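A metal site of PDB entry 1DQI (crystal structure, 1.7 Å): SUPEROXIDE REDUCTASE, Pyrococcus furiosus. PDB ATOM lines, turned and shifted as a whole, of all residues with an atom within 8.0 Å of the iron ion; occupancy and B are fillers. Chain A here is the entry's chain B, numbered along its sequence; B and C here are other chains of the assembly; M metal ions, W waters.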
ATOM      1  N   HIS A  16      -7.972 -15.798  -5.234  1.00  0.00           N
ATOM      2  CA  HIS A  16      -9.248 -15.415  -4.643  1.00  0.00           C
ATOM      3  C   HIS A  16      -9.771 -14.104  -5.212  1.00  0.00           C
ATOM      4  O   HIS A  16     -10.976 -13.931  -5.372  1.00  0.00           O
ATOM      5  CB  HIS A  16      -9.102 -15.277  -3.120  1.00  0.00           C
ATOM      6  CG  HIS A  16      -9.247 -16.567  -2.387  1.00  0.00           C
ATOM      7  ND1 HIS A  16      -8.277 -17.076  -1.544  1.00  0.00           N
ATOM      8  CD2 HIS A  16     -10.275 -17.456  -2.353  1.00  0.00           C
ATOM      9  CE1 HIS A  16      -8.746 -18.234  -1.040  1.00  0.00           C
ATOM     10  NE2 HIS A  16      -9.943 -18.506  -1.500  1.00  0.00           N
ATOM     11  N   VAL A  35     -12.218 -15.840 -11.017  1.00  0.00           N
ATOM     12  CA  VAL A  35     -11.389 -16.085  -9.846  1.00  0.00           C
ATOM     13  C   VAL A  35     -10.506 -17.274 -10.214  1.00  0.00           C
ATOM     14  O   VAL A  35     -10.995 -18.279 -10.711  1.00  0.00           O
ATOM     15  CB  VAL A  35     -12.237 -16.460  -8.612  1.00  0.00           C
ATOM     16  CG1 VAL A  35     -11.330 -16.908  -7.474  1.00  0.00           C
ATOM     17  CG2 VAL A  35     -13.085 -15.282  -8.183  1.00  0.00           C
ATOM     18  N   HIS A  41      -8.400 -21.663  -8.573  1.00  0.00           N
ATOM     19  CA  HIS A  41      -8.947 -21.843  -7.242  1.00  0.00           C
ATOM     20  C   HIS A  41      -9.602 -23.221  -7.203  1.00  0.00           C
ATOM     21  O   HIS A  41     -10.184 -23.672  -8.180  1.00  0.00           O
ATOM     22  CB  HIS A  41      -9.993 -20.761  -6.936  1.00  0.00           C
ATOM     23  CG  HIS A  41     -10.543 -20.833  -5.546  1.00  0.00           C
ATOM     24  ND1 HIS A  41     -11.558 -21.679  -5.166  1.00  0.00           N
ATOM     25  CD2 HIS A  41     -10.204 -20.144  -4.430  1.00  0.00           C
ATOM     26  CE1 HIS A  41     -11.797 -21.478  -3.854  1.00  0.00           C
ATOM     27  NE2 HIS A  41     -10.995 -20.557  -3.364  1.00  0.00           N
ATOM     28  N   PRO A  42      -9.495 -23.921  -6.065  1.00  0.00           N
ATOM     29  CA  PRO A  42     -10.119 -25.243  -6.004  1.00  0.00           C
ATOM     30  C   PRO A  42     -11.627 -25.140  -6.261  1.00  0.00           C
ATOM     31  O   PRO A  42     -12.245 -24.124  -5.967  1.00  0.00           O
ATOM     32  CB  PRO A  42      -9.819 -25.731  -4.588  1.00  0.00           C
ATOM     33  CG  PRO A  42      -8.672 -24.906  -4.121  1.00  0.00           C
ATOM     34  CD  PRO A  42      -8.817 -23.575  -4.796  1.00  0.00           C
ATOM     35  N   GLU A  46     -16.199 -29.319  -0.966  1.00  0.00           N
ATOM     36  CA  GLU A  46     -15.816 -28.701   0.300  1.00  0.00           C
ATOM     37  C   GLU A  46     -15.289 -27.277   0.199  1.00  0.00           C
ATOM     38  O   GLU A  46     -15.387 -26.499   1.153  1.00  0.00           O
ATOM     39  CB  GLU A  46     -14.754 -29.572   0.983  1.00  0.00           C
ATOM     40  CG  GLU A  46     -15.209 -30.984   1.313  1.00  0.00           C
ATOM     41  CD  GLU A  46     -14.958 -31.973   0.182  1.00  0.00           C
ATOM     42  OE1 GLU A  46     -15.201 -33.179   0.404  1.00  0.00           O
ATOM     43  OE2 GLU A  46     -14.520 -31.550  -0.905  1.00  0.00           O
ATOM     44  N   HIS A  47     -14.736 -26.935  -0.957  1.00  0.00           N
ATOM     45  CA  HIS A  47     -14.118 -25.621  -1.142  1.00  0.00           C
ATOM     46  C   HIS A  47     -14.363 -25.094  -2.557  1.00  0.00           C
ATOM     47  O   HIS A  47     -13.851 -25.655  -3.520  1.00  0.00           O
ATOM     48  CB  HIS A  47     -12.619 -25.769  -0.869  1.00  0.00           C
ATOM     49  CG  HIS A  47     -11.856 -24.493  -0.884  1.00  0.00           C
ATOM     50  ND1 HIS A  47     -10.479 -24.424  -0.871  1.00  0.00           N
ATOM     51  CD2 HIS A  47     -12.290 -23.206  -0.886  1.00  0.00           C
ATOM     52  CE1 HIS A  47     -10.137 -23.127  -0.881  1.00  0.00           C
ATOM     53  NE2 HIS A  47     -11.192 -22.353  -0.885  1.00  0.00           N
ATOM     54  N   HIS A  48     -15.124 -24.008  -2.673  1.00  0.00           N
ATOM     55  CA  HIS A  48     -15.441 -23.452  -3.991  1.00  0.00           C
ATOM     56  C   HIS A  48     -15.916 -22.005  -3.971  1.00  0.00           C
ATOM     57  O   HIS A  48     -16.324 -21.473  -2.926  1.00  0.00           O
ATOM     58  CB  HIS A  48     -16.518 -24.304  -4.654  1.00  0.00           C
ATOM     59  CG  HIS A  48     -17.746 -24.482  -3.795  1.00  0.00           C
ATOM     60  ND1 HIS A  48     -17.982 -25.638  -3.085  1.00  0.00           N
ATOM     61  CD2 HIS A  48     -18.771 -23.651  -3.513  1.00  0.00           C
ATOM     62  CE1 HIS A  48     -19.113 -25.501  -2.399  1.00  0.00           C
ATOM     63  NE2 HIS A  48     -19.600 -24.302  -2.643  1.00  0.00           N
ATOM     64  N   ILE A  49     -15.868 -21.378  -5.139  1.00  0.00           N
ATOM     65  CA  ILE A  49     -16.349 -20.003  -5.304  1.00  0.00           C
ATOM     66  C   ILE A  49     -17.848 -20.155  -5.582  1.00  0.00           C
ATOM     67  O   ILE A  49     -18.243 -20.861  -6.518  1.00  0.00           O
ATOM     68  CB  ILE A  49     -15.668 -19.316  -6.503  1.00  0.00           C
ATOM     69  CG1 ILE A  49     -14.149 -19.281  -6.299  1.00  0.00           C
ATOM     70  CG2 ILE A  49     -16.223 -17.899  -6.682  1.00  0.00           C
ATOM     71  CD1 ILE A  49     -13.701 -18.517  -5.072  1.00  0.00           C
ATOM     72  N   TYR A 110     -17.579 -14.532  -3.523  1.00  0.00           N
ATOM     73  CA  TYR A 110     -17.660 -15.197  -2.245  1.00  0.00           C
ATOM     74  C   TYR A 110     -17.156 -16.631  -2.342  1.00  0.00           C
ATOM     75  O   TYR A 110     -17.626 -17.401  -3.185  1.00  0.00           O
ATOM     76  CB  TYR A 110     -19.115 -15.206  -1.755  1.00  0.00           C
ATOM     77  CG  TYR A 110     -19.315 -15.957  -0.462  1.00  0.00           C
ATOM     78  CD1 TYR A 110     -18.781 -15.472   0.736  1.00  0.00           C
ATOM     79  CD2 TYR A 110     -20.019 -17.154  -0.430  1.00  0.00           C
ATOM     80  CE1 TYR A 110     -18.959 -16.162   1.935  1.00  0.00           C
ATOM     81  CE2 TYR A 110     -20.197 -17.866   0.770  1.00  0.00           C
ATOM     82  CZ  TYR A 110     -19.657 -17.350   1.948  1.00  0.00           C
ATOM     83  OH  TYR A 110     -19.811 -18.035   3.127  1.00  0.00           O
ATOM     84  N   CYS A 111     -16.198 -16.957  -1.482  1.00  0.00           N
ATOM     85  CA  CYS A 111     -15.638 -18.300  -1.406  1.00  0.00           C
ATOM     86  C   CYS A 111     -16.381 -18.918  -0.225  1.00  0.00           C
ATOM     87  O   CYS A 111     -16.588 -18.243   0.788  1.00  0.00           O
ATOM     88  CB  CYS A 111     -14.138 -18.259  -1.118  1.00  0.00           C
ATOM     89  SG  CYS A 111     -13.420 -19.903  -0.808  1.00  0.00           S
ATOM     90  N   ASN A 112     -16.785 -20.175  -0.329  1.00  0.00           N
ATOM     91  CA  ASN A 112     -17.552 -20.779   0.751  1.00  0.00           C
ATOM     92  C   ASN A 112     -16.839 -20.909   2.100  1.00  0.00           C
ATOM     93  O   ASN A 112     -17.505 -21.035   3.121  1.00  0.00           O
ATOM     94  CB  ASN A 112     -18.128 -22.132   0.302  1.00  0.00           C
ATOM     95  CG  ASN A 112     -17.091 -23.226   0.266  1.00  0.00           C
ATOM     96  OD1 ASN A 112     -15.921 -22.990  -0.016  1.00  0.00           O
ATOM     97  ND2 ASN A 112     -17.521 -24.458   0.543  1.00  0.00           N
ATOM     98  N   ILE A 113     -15.503 -20.860   2.109  1.00  0.00           N
ATOM     99  CA  ILE A 113     -14.773 -20.951   3.372  1.00  0.00           C
ATOM    100  C   ILE A 113     -13.761 -19.824   3.571  1.00  0.00           C
ATOM    101  O   ILE A 113     -13.194 -19.680   4.655  1.00  0.00           O
ATOM    102  CB  ILE A 113     -14.009 -22.296   3.500  1.00  0.00           C
ATOM    103  CG1 ILE A 113     -12.980 -22.433   2.371  1.00  0.00           C
ATOM    104  CG2 ILE A 113     -14.988 -23.470   3.504  1.00  0.00           C
ATOM    105  CD1 ILE A 113     -12.055 -23.641   2.512  1.00  0.00           C
ATOM    106  N   HIS A 114     -13.548 -19.008   2.541  1.00  0.00           N
ATOM    107  CA  HIS A 114     -12.578 -17.922   2.639  1.00  0.00           C
ATOM    108  C   HIS A 114     -13.161 -16.517   2.574  1.00  0.00           C
ATOM    109  O   HIS A 114     -12.450 -15.564   2.266  1.00  0.00           O
ATOM    110  CB  HIS A 114     -11.499 -18.087   1.568  1.00  0.00           C
ATOM    111  CG  HIS A 114     -10.553 -19.219   1.845  1.00  0.00           C
ATOM    112  ND1 HIS A 114     -10.142 -20.076   0.859  1.00  0.00           N
ATOM    113  CD2 HIS A 114      -9.980 -19.583   3.023  1.00  0.00           C
ATOM    114  CE1 HIS A 114      -9.337 -20.939   1.441  1.00  0.00           C
ATOM    115  NE2 HIS A 114      -9.198 -20.685   2.756  1.00  0.00           N
ATOM    116  N   GLY A 115     -14.452 -16.392   2.874  1.00  0.00           N
ATOM    117  CA  GLY A 115     -15.102 -15.097   2.895  1.00  0.00           C
ATOM    118  C   GLY A 115     -15.311 -14.346   1.592  1.00  0.00           C
ATOM    119  O   GLY A 115     -15.285 -14.915   0.493  1.00  0.00           O
ATOM    120  N   TRP A 117     -14.450 -11.359  -1.284  1.00  0.00           N
ATOM    121  CA  TRP A 117     -13.302 -10.792  -1.988  1.00  0.00           C
ATOM    122  C   TRP A 117     -13.770  -9.747  -2.981  1.00  0.00           C
ATOM    123  O   TRP A 117     -14.864  -9.859  -3.527  1.00  0.00           O
ATOM    124  CB  TRP A 117     -12.540 -11.905  -2.703  1.00  0.00           C
ATOM    125  CG  TRP A 117     -11.892 -12.830  -1.745  1.00  0.00           C
ATOM    126  CD1 TRP A 117     -12.480 -13.882  -1.091  1.00  0.00           C
ATOM    127  CD2 TRP A 117     -10.533 -12.784  -1.298  1.00  0.00           C
ATOM    128  NE1 TRP A 117     -11.566 -14.480  -0.263  1.00  0.00           N
ATOM    129  CE2 TRP A 117     -10.369 -13.830  -0.366  1.00  0.00           C
ATOM    130  CE3 TRP A 117      -9.441 -11.955  -1.591  1.00  0.00           C
ATOM    131  CZ2 TRP A 117      -9.145 -14.064   0.276  1.00  0.00           C
ATOM    132  CZ3 TRP A 117      -8.230 -12.194  -0.945  1.00  0.00           C
ATOM    133  CH2 TRP A 117      -8.097 -13.247  -0.022  1.00  0.00           C
ATOM    134  N   VAL B  79     -12.413 -23.757   6.806  1.00  0.00           N
ATOM    135  CA  VAL B  79     -11.034 -24.072   6.465  1.00  0.00           C
ATOM    136  C   VAL B  79     -10.568 -25.301   7.238  1.00  0.00           C
ATOM    137  O   VAL B  79      -9.539 -25.891   6.913  1.00  0.00           O
ATOM    138  CB  VAL B  79     -10.084 -22.901   6.792  1.00  0.00           C
ATOM    139  CG1 VAL B  79     -10.393 -21.712   5.909  1.00  0.00           C
ATOM    140  CG2 VAL B  79     -10.202 -22.525   8.261  1.00  0.00           C
ATOM    141  N   PHE C  63     -12.844 -15.623   8.658  1.00  0.00           N
ATOM    142  CA  PHE C  63     -13.653 -15.633   7.449  1.00  0.00           C
ATOM    143  C   PHE C  63     -15.148 -15.560   7.672  1.00  0.00           C
ATOM    144  O   PHE C  63     -15.744 -16.406   8.335  1.00  0.00           O
ATOM    145  CB  PHE C  63     -13.298 -16.879   6.627  1.00  0.00           C
ATOM    146  CG  PHE C  63     -11.824 -16.978   6.317  1.00  0.00           C
ATOM    147  CD1 PHE C  63     -11.044 -17.982   6.894  1.00  0.00           C
ATOM    148  CD2 PHE C  63     -11.220 -16.059   5.467  1.00  0.00           C
ATOM    149  CE1 PHE C  63      -9.669 -18.058   6.626  1.00  0.00           C
ATOM    150  CE2 PHE C  63      -9.851 -16.131   5.183  1.00  0.00           C
ATOM    151  CZ  PHE C  63      -9.077 -17.135   5.768  1.00  0.00           C
HETATM  152 FE    FE M   1     -10.821 -20.416  -1.170  1.00  0.00          FE
HETATM  153  O   HOH W   1      -8.350 -21.053  -1.404  1.00  0.00           O
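The backbone NH (N) of Ile 113 lies close to the side-chain sulfur (SG) of Cys 111, at 3.7 Å.
The indole nitrogen (NE1) of Trp 117 is in hydrogen-bond range of the backbone carbonyl oxygen (O) of His 114 (2.9 Å).
Five residues have an atom within 4 Å of the iron ion: His 16, His 41, His 47, Cys 111 and His 114.
The iron ion is bound by NE2 of His 47 (2.0 Å), NE2 of His 16 (2.1 Å), ND1 of His 114 (2.2 Å), NE2 of His 41 (2.2 Å), water W1 (2.6 Å) and SG of Cys 111 (2.7 Å).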
